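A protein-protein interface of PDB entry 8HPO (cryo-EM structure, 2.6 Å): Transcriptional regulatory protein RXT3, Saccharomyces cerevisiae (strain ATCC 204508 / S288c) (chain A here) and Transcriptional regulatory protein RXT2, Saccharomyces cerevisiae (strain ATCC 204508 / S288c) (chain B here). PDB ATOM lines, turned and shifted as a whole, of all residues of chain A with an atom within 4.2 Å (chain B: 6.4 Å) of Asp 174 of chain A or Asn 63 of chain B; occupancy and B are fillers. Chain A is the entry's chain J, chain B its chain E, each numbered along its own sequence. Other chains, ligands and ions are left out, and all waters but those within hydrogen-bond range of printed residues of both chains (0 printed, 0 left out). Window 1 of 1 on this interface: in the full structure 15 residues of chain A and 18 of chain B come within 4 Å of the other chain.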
ATOM      1  N   GLU A 164       6.022  15.038   1.921  1.00  0.00           N
ATOM      2  CA  GLU A 164       5.431  15.896   0.893  1.00  0.00           C
ATOM      3  C   GLU A 164       4.123  16.499   1.396  1.00  0.00           C
ATOM      4  O   GLU A 164       3.028  16.005   1.125  1.00  0.00           O
ATOM      5  CB  GLU A 164       5.211  15.111  -0.392  1.00  0.00           C
ATOM      6  CG  GLU A 164       6.456  14.465  -0.956  1.00  0.00           C
ATOM      7  CD  GLU A 164       6.268  14.021  -2.386  1.00  0.00           C
ATOM      8  OE1 GLU A 164       6.787  12.947  -2.760  1.00  0.00           O
ATOM      9  OE2 GLU A 164       5.596  14.745  -3.143  1.00  0.00           O
ATOM     10  N   TRP A 166       2.631  20.721   2.208  1.00  0.00           N
ATOM     11  CA  TRP A 166       2.894  22.159   2.215  1.00  0.00           C
ATOM     12  C   TRP A 166       1.637  22.904   2.636  1.00  0.00           C
ATOM     13  O   TRP A 166       0.610  22.823   1.954  1.00  0.00           O
ATOM     14  CB  TRP A 166       3.362  22.649   0.835  1.00  0.00           C
ATOM     15  CG  TRP A 166       4.727  22.184   0.483  1.00  0.00           C
ATOM     16  CD1 TRP A 166       5.902  22.766   0.832  1.00  0.00           C
ATOM     17  CD2 TRP A 166       5.064  21.016  -0.266  1.00  0.00           C
ATOM     18  NE1 TRP A 166       6.954  22.039   0.342  1.00  0.00           N
ATOM     19  CE2 TRP A 166       6.463  20.953  -0.333  1.00  0.00           C
ATOM     20  CE3 TRP A 166       4.316  20.015  -0.884  1.00  0.00           C
ATOM     21  CZ2 TRP A 166       7.128  19.933  -0.994  1.00  0.00           C
ATOM     22  CZ3 TRP A 166       4.981  19.008  -1.541  1.00  0.00           C
ATOM     23  CH2 TRP A 166       6.368  18.974  -1.593  1.00  0.00           C
ATOM     24  N   SER A 172      -1.037  22.700  -1.009  1.00  0.00           N
ATOM     25  CA  SER A 172      -0.757  22.648  -2.433  1.00  0.00           C
ATOM     26  C   SER A 172      -1.302  21.362  -3.029  1.00  0.00           C
ATOM     27  O   SER A 172      -1.688  20.435  -2.321  1.00  0.00           O
ATOM     28  CB  SER A 172       0.745  22.712  -2.692  1.00  0.00           C
ATOM     29  OG  SER A 172       1.399  23.501  -1.722  1.00  0.00           O
ATOM     30  N   ASP A 173      -1.311  21.304  -4.356  1.00  0.00           N
ATOM     31  CA  ASP A 173      -1.611  20.053  -5.035  1.00  0.00           C
ATOM     32  C   ASP A 173      -0.438  19.087  -5.018  1.00  0.00           C
ATOM     33  O   ASP A 173      -0.507  18.040  -5.667  1.00  0.00           O
ATOM     34  CB  ASP A 173      -2.036  20.328  -6.474  1.00  0.00           C
ATOM     35  CG  ASP A 173      -3.513  20.617  -6.594  1.00  0.00           C
ATOM     36  OD1 ASP A 173      -4.177  19.997  -7.452  1.00  0.00           O
ATOM     37  OD2 ASP A 173      -4.014  21.458  -5.825  1.00  0.00           O
ATOM     38  N   ASP A 174       0.633  19.418  -4.302  1.00  0.00           N
ATOM     39  CA  ASP A 174       1.787  18.550  -4.138  1.00  0.00           C
ATOM     40  C   ASP A 174       1.847  17.919  -2.757  1.00  0.00           C
ATOM     41  O   ASP A 174       2.762  17.138  -2.486  1.00  0.00           O
ATOM     42  CB  ASP A 174       3.074  19.331  -4.399  1.00  0.00           C
ATOM     43  CG  ASP A 174       3.058  20.042  -5.716  1.00  0.00           C
ATOM     44  OD1 ASP A 174       2.060  19.904  -6.445  1.00  0.00           O
ATOM     45  OD2 ASP A 174       4.043  20.744  -6.020  1.00  0.00           O
ATOM     46  N   SER A 175       0.907  18.251  -1.878  1.00  0.00           N
ATOM     47  CA  SER A 175       0.825  17.637  -0.562  1.00  0.00           C
ATOM     48  C   SER A 175      -0.005  16.363  -0.640  1.00  0.00           C
ATOM     49  O   SER A 175      -1.077  16.344  -1.246  1.00  0.00           O
ATOM     50  CB  SER A 175       0.213  18.607   0.451  1.00  0.00           C
ATOM     51  OG  SER A 175       0.962  19.807   0.539  1.00  0.00           O
ATOM     52  N   ASP A 176       0.502  15.301  -0.027  1.00  0.00           N
ATOM     53  CA  ASP A 176      -0.151  14.005  -0.132  1.00  0.00           C
ATOM     54  C   ASP A 176      -1.463  14.003   0.649  1.00  0.00           C
ATOM     55  O   ASP A 176      -1.554  14.628   1.711  1.00  0.00           O
ATOM     56  CB  ASP A 176       0.774  12.905   0.388  1.00  0.00           C
ATOM     57  CG  ASP A 176       0.377  11.525  -0.101  1.00  0.00           C
ATOM     58  OD1 ASP A 176      -0.786  11.120   0.078  1.00  0.00           O
ATOM     59  OD2 ASP A 176       1.233  10.841  -0.687  1.00  0.00           O
ATOM     60  N   TRP A 252       6.214  26.961   1.744  1.00  0.00           N
ATOM     61  CA  TRP A 252       6.310  27.431   0.365  1.00  0.00           C
ATOM     62  C   TRP A 252       5.516  28.720   0.237  1.00  0.00           C
ATOM     63  O   TRP A 252       4.296  28.715   0.411  1.00  0.00           O
ATOM     64  CB  TRP A 252       5.781  26.389  -0.622  1.00  0.00           C
ATOM     65  CG  TRP A 252       6.158  26.653  -2.047  1.00  0.00           C
ATOM     66  CD1 TRP A 252       5.387  27.239  -3.002  1.00  0.00           C
ATOM     67  CD2 TRP A 252       7.397  26.321  -2.680  1.00  0.00           C
ATOM     68  NE1 TRP A 252       6.071  27.306  -4.185  1.00  0.00           N
ATOM     69  CE2 TRP A 252       7.308  26.743  -4.014  1.00  0.00           C
ATOM     70  CE3 TRP A 252       8.576  25.712  -2.243  1.00  0.00           C
ATOM     71  CZ2 TRP A 252       8.350  26.575  -4.913  1.00  0.00           C
ATOM     72  CZ3 TRP A 252       9.604  25.549  -3.139  1.00  0.00           C
ATOM     73  CH2 TRP A 252       9.485  25.973  -4.457  1.00  0.00           C
ATOM     74  N   HIS A 260       3.137  29.288  -5.927  1.00  0.00           N
ATOM     75  CA  HIS A 260       2.890  27.895  -6.266  1.00  0.00           C
ATOM     76  C   HIS A 260       2.146  27.790  -7.590  1.00  0.00           C
ATOM     77  O   HIS A 260       1.302  28.624  -7.924  1.00  0.00           O
ATOM     78  CB  HIS A 260       2.089  27.206  -5.165  1.00  0.00           C
ATOM     79  CG  HIS A 260       1.579  25.856  -5.554  1.00  0.00           C
ATOM     80  ND1 HIS A 260       0.249  25.601  -5.798  1.00  0.00           N
ATOM     81  CD2 HIS A 260       2.230  24.692  -5.772  1.00  0.00           C
ATOM     82  CE1 HIS A 260       0.099  24.333  -6.132  1.00  0.00           C
ATOM     83  NE2 HIS A 260       1.289  23.760  -6.128  1.00  0.00           N
ATOM     84  N   ASP A 261       2.455  26.737  -8.339  1.00  0.00           N
ATOM     85  CA  ASP A 261       1.977  26.621  -9.710  1.00  0.00           C
ATOM     86  C   ASP A 261       0.501  26.243  -9.776  1.00  0.00           C
ATOM     87  O   ASP A 261      -0.312  26.985 -10.336  1.00  0.00           O
ATOM     88  CB  ASP A 261       2.839  25.606 -10.454  1.00  0.00           C
ATOM     89  CG  ASP A 261       4.315  25.894 -10.298  1.00  0.00           C
ATOM     90  OD1 ASP A 261       4.767  26.073  -9.146  1.00  0.00           O
ATOM     91  OD2 ASP A 261       5.026  25.951 -11.322  1.00  0.00           O
ATOM     92  N   ILE B  60      14.571  21.948 -14.756  1.00  0.00           N
ATOM     93  CA  ILE B  60      13.123  21.902 -14.609  1.00  0.00           C
ATOM     94  C   ILE B  60      12.527  23.203 -15.123  1.00  0.00           C
ATOM     95  O   ILE B  60      13.126  24.273 -14.987  1.00  0.00           O
ATOM     96  CB  ILE B  60      12.733  21.648 -13.142  1.00  0.00           C
ATOM     97  CG1 ILE B  60      13.614  22.470 -12.207  1.00  0.00           C
ATOM     98  CG2 ILE B  60      12.853  20.183 -12.811  1.00  0.00           C
ATOM     99  CD1 ILE B  60      12.898  22.938 -10.973  1.00  0.00           C
ATOM    100  N   SER B  61      11.341  23.112 -15.718  1.00  0.00           N
ATOM    101  CA  SER B  61      10.638  24.291 -16.211  1.00  0.00           C
ATOM    102  C   SER B  61       9.510  24.693 -15.267  1.00  0.00           C
ATOM    103  O   SER B  61       9.404  25.857 -14.875  1.00  0.00           O
ATOM    104  CB  SER B  61      10.092  24.035 -17.618  1.00  0.00           C
ATOM    105  OG  SER B  61       8.709  23.736 -17.576  1.00  0.00           O
ATOM    106  N   SER B  62       8.659  23.740 -14.901  1.00  0.00           N
ATOM    107  CA  SER B  62       7.601  23.990 -13.939  1.00  0.00           C
ATOM    108  C   SER B  62       8.113  23.759 -12.524  1.00  0.00           C
ATOM    109  O   SER B  62       9.295  23.501 -12.288  1.00  0.00           O
ATOM    110  CB  SER B  62       6.396  23.101 -14.227  1.00  0.00           C
ATOM    111  OG  SER B  62       5.370  23.310 -13.278  1.00  0.00           O
ATOM    112  N   ASN B  63       7.212  23.858 -11.562  1.00  0.00           N
ATOM    113  CA  ASN B  63       7.575  23.596 -10.181  1.00  0.00           C
ATOM    114  C   ASN B  63       6.573  22.713  -9.456  1.00  0.00           C
ATOM    115  O   ASN B  63       6.843  22.314  -8.322  1.00  0.00           O
ATOM    116  CB  ASN B  63       7.738  24.911  -9.420  1.00  0.00           C
ATOM    117  CG  ASN B  63       8.539  24.750  -8.172  1.00  0.00           C
ATOM    118  OD1 ASN B  63       9.758  24.864  -8.187  1.00  0.00           O
ATOM    119  ND2 ASN B  63       7.863  24.456  -7.079  1.00  0.00           N
ATOM    120  N   ARG B  64       5.433  22.401 -10.061  1.00  0.00           N
ATOM    121  CA  ARG B  64       4.480  21.481  -9.460  1.00  0.00           C
ATOM    122  C   ARG B  64       5.037  20.068  -9.552  1.00  0.00           C
ATOM    123  O   ARG B  64       5.134  19.505 -10.646  1.00  0.00           O
ATOM    124  CB  ARG B  64       3.131  21.571 -10.162  1.00  0.00           C
ATOM    125  CG  ARG B  64       2.254  20.372  -9.912  1.00  0.00           C
ATOM    126  CD  ARG B  64       1.178  20.230 -10.958  1.00  0.00           C
ATOM    127  NE  ARG B  64       0.030  19.498 -10.434  1.00  0.00           N
ATOM    128  CZ  ARG B  64      -0.017  18.178 -10.297  1.00  0.00           C
ATOM    129  NH1 ARG B  64      -1.103  17.601  -9.807  1.00  0.00           N
ATOM    130  NH2 ARG B  64       1.019  17.435 -10.652  1.00  0.00           N
ATOM    131  N   GLY B  65       5.414  19.501  -8.410  1.00  0.00           N
ATOM    132  CA  GLY B  65       6.021  18.193  -8.362  1.00  0.00           C
ATOM    133  C   GLY B  65       7.526  18.200  -8.239  1.00  0.00           C
ATOM    134  O   GLY B  65       8.142  17.133  -8.335  1.00  0.00           O
ATOM    135  N   ASN B  66       8.136  19.361  -8.036  1.00  0.00           N
ATOM    136  CA  ASN B  66       9.586  19.497  -7.988  1.00  0.00           C
ATOM    137  C   ASN B  66      10.006  20.385  -6.828  1.00  0.00           C
ATOM    138  O   ASN B  66      11.054  21.034  -6.866  1.00  0.00           O
ATOM    139  CB  ASN B  66      10.122  20.052  -9.304  1.00  0.00           C
ATOM    140  CG  ASN B  66       9.773  19.179 -10.494  1.00  0.00           C
ATOM    141  OD1 ASN B  66       8.668  19.248 -11.029  1.00  0.00           O
ATOM    142  ND2 ASN B  66      10.719  18.352 -10.916  1.00  0.00           N
ATOM    143  N   LYS B  67       9.188  20.423  -5.777  1.00  0.00           N
ATOM    144  CA  LYS B  67       9.450  21.335  -4.671  1.00  0.00           C
ATOM    145  C   LYS B  67      10.578  20.843  -3.778  1.00  0.00           C
ATOM    146  O   LYS B  67      11.151  21.626  -3.015  1.00  0.00           O
ATOM    147  CB  LYS B  67       8.194  21.528  -3.834  1.00  0.00           C
ATOM    148  CG  LYS B  67       7.033  22.137  -4.561  1.00  0.00           C
ATOM    149  CD  LYS B  67       6.366  23.171  -3.693  1.00  0.00           C
ATOM    150  CE  LYS B  67       5.141  23.718  -4.358  1.00  0.00           C
ATOM    151  NZ  LYS B  67       4.260  22.633  -4.804  1.00  0.00           N
ATOM    152  N   SER B  72      15.063  25.097  -6.416  1.00  0.00           N
ATOM    153  CA  SER B  72      13.785  25.109  -7.118  1.00  0.00           C
ATOM    154  C   SER B  72      12.834  26.211  -6.667  1.00  0.00           C
ATOM    155  O   SER B  72      11.827  26.467  -7.331  1.00  0.00           O
ATOM    156  CB  SER B  72      13.097  23.760  -6.925  1.00  0.00           C
ATOM    157  OG  SER B  72      11.951  23.636  -7.741  1.00  0.00           O
ATOM    158  N   GLU B  73      13.108  26.835  -5.524  1.00  0.00           N
ATOM    159  CA  GLU B  73      12.302  27.942  -5.025  1.00  0.00           C
ATOM    160  C   GLU B  73      12.092  29.029  -6.073  1.00  0.00           C
ATOM    161  O   GLU B  73      11.095  29.755  -6.030  1.00  0.00           O
ATOM    162  CB  GLU B  73      12.960  28.553  -3.790  1.00  0.00           C
ATOM    163  CG  GLU B  73      13.195  27.571  -2.666  1.00  0.00           C
ATOM    164  CD  GLU B  73      14.664  27.408  -2.343  1.00  0.00           C
ATOM    165  OE1 GLU B  73      15.468  28.234  -2.822  1.00  0.00           O
ATOM    166  OE2 GLU B  73      15.018  26.457  -1.614  1.00  0.00           O
ATOM    167  N   VAL B  74      13.021  29.139  -7.021  1.00  0.00           N
ATOM    168  CA  VAL B  74      13.080  30.261  -7.951  1.00  0.00           C
ATOM    169  C   VAL B  74      12.686  29.848  -9.362  1.00  0.00           C
ATOM    170  O   VAL B  74      13.144  30.450 -10.336  1.00  0.00           O
ATOM    171  CB  VAL B  74      14.487  30.873  -7.945  1.00  0.00           C
ATOM    172  CG1 VAL B  74      14.835  31.355  -6.563  1.00  0.00           C
ATOM    173  CG2 VAL B  74      15.482  29.842  -8.371  1.00  0.00           C
ATOM    174  N   VAL B  75      11.841  28.828  -9.492  1.00  0.00           N
ATOM    175  CA  VAL B  75      11.426  28.309 -10.790  1.00  0.00           C
ATOM    176  C   VAL B  75       9.912  28.394 -10.897  1.00  0.00           C
ATOM    177  O   VAL B  75       9.193  27.859 -10.049  1.00  0.00           O
ATOM    178  CB  VAL B  75      11.904  26.863 -10.998  1.00  0.00           C
ATOM    179  CG1 VAL B  75      11.433  26.352 -12.335  1.00  0.00           C
ATOM    180  CG2 VAL B  75      13.412  26.788 -10.913  1.00  0.00           C
ATOM    181  N   THR B  76       9.430  29.047 -11.951  1.00  0.00           N
ATOM    182  CA  THR B  76       8.008  29.170 -12.231  1.00  0.00           C
ATOM    183  C   THR B  76       7.731  28.713 -13.652  1.00  0.00           C
ATOM    184  O   THR B  76       8.623  28.707 -14.502  1.00  0.00           O
ATOM    185  CB  THR B  76       7.519  30.607 -12.089  1.00  0.00           C
ATOM    186  OG1 THR B  76       8.297  31.281 -11.100  1.00  0.00           O
ATOM    187  CG2 THR B  76       6.061  30.632 -11.678  1.00  0.00           C
ATOM    188  N   ARG B  77       6.482  28.345 -13.911  1.00  0.00           N
ATOM    189  CA  ARG B  77       6.026  28.032 -15.255  1.00  0.00           C
ATOM    190  C   ARG B  77       5.531  29.261 -15.998  1.00  0.00           C
ATOM    191  O   ARG B  77       4.960  29.128 -17.085  1.00  0.00           O
ATOM    192  CB  ARG B  77       4.916  26.988 -15.205  1.00  0.00           C
ATOM    193  CG  ARG B  77       3.919  27.245 -14.106  1.00  0.00           C
ATOM    194  CD  ARG B  77       2.649  26.483 -14.344  1.00  0.00           C
ATOM    195  NE  ARG B  77       2.876  25.053 -14.219  1.00  0.00           N
ATOM    196  CZ  ARG B  77       1.960  24.189 -13.809  1.00  0.00           C
ATOM    197  NH1 ARG B  77       2.256  22.902 -13.729  1.00  0.00           N
ATOM    198  NH2 ARG B  77       0.750  24.615 -13.476  1.00  0.00           N
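The backbone NH (N) of Arg 64 of chain B sits at hydrogen-bond distance from the side-chain hydroxyl (OG) of Ser 62 of chain B (3.3 Å). The backbone carbonyl oxygen (O) of Trp 166 of chain A lies within hydrogen-bond range of the backbone NH (N) of Ser 172 of chain A (3.4 Å). The side-chain hydroxyl (OG) of Ser 72 of chain B lies within hydrogen-bond range of the side-chain amide oxygen (OD1) of Asn 63 of chain B. The side-chain hydroxyl (OG) of Ser 72 of chain B is in hydrogen-bond range of the backbone carbonyl oxygen (O) of Asn 66 of chain B (2.9 Å). The backbone NH (N) of Trp 166 of chain A is in hydrogen-bond range of the side-chain hydroxyl (OG) of Ser 175 of chain A (2.5 Å). OG of Ser 62 of chain B is in hydrogen-bond range of NH1 of Arg 77 of chain B.
Among the printed residues, Asp or Glu carboxylates within 4 Å of a Lys or Arg side-chain nitrogen of the other chain: Asp 174 of chain A with Lys 67 of chain B (2.3 Å) and Asp 261 of chain A with Arg 77 of chain B (3.7 Å).
The backbone NH (N) of Gly 65 of chain B lies within hydrogen-bond range of the side-chain carboxylate (OD2) of Asp 174 of chain A. OD2 of Asp 261 of chain A sits at hydrogen-bond distance from OG of Ser 62 of chain B. N of Asn 63 of chain B is in hydrogen-bond range of OD2 of Asp 261 of chain A, at 3.0 Å. A ring nitrogen (NE2) of His 260 of chain A sits close to the side-chain amino group (NZ) of Lys 67 of chain B. OD2 of Asp 261 of chain A is in salt-bridge range of NE of Arg 77 of chain B, at 3.7 Å. OD1 of Asp 174 of chain A is in salt-bridge range of NZ of Lys 67 of chain B (3.9 Å).
Trp 166 of chain A touches Lys 67 of chain B (CZ2 to CB, 3.4 Å). O of Asn 63 of chain B touches OD2 of Asp 174 of chain A (3.95 Å). CG of Arg 64 of chain B touches OD1 of Asp 174 of chain A (3.5 Å). Asn 63 of chain B touches Trp 252 of chain A. CD of Lys 67 of chain B touches CD2 of Trp 252 of chain A (3.5 Å). CH2 of Trp 252 of chain A touches O of Ser 72 of chain B, 3.7 Å away. CH2 of Trp 252 of chain A touches CA of Glu 73 of chain B, at 3.5 Å. Arg 64 of chain B touches Asp 261 of chain A (N to CG, 3.7 Å).
Of the printed residues of chain B, Asp 174 of chain A touches Asn 63, Arg 64, Gly 65 and Lys 67. Asn 63 of chain B touches just these residues of chain A: Asp 174, Trp 252 and Asp 261. Of the printed residues of chain A, Ser 72 of chain B touches Trp 252 (3.7 Å). Of the printed residues of chain A, Gly 65 of chain B touches Asp 174. Val 75 of chain B touches none of the printed residues of chain A. The nearest residue of chain B that does not touch Asp 174 of chain A is Asn 66 of chain B (4.8 Å).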
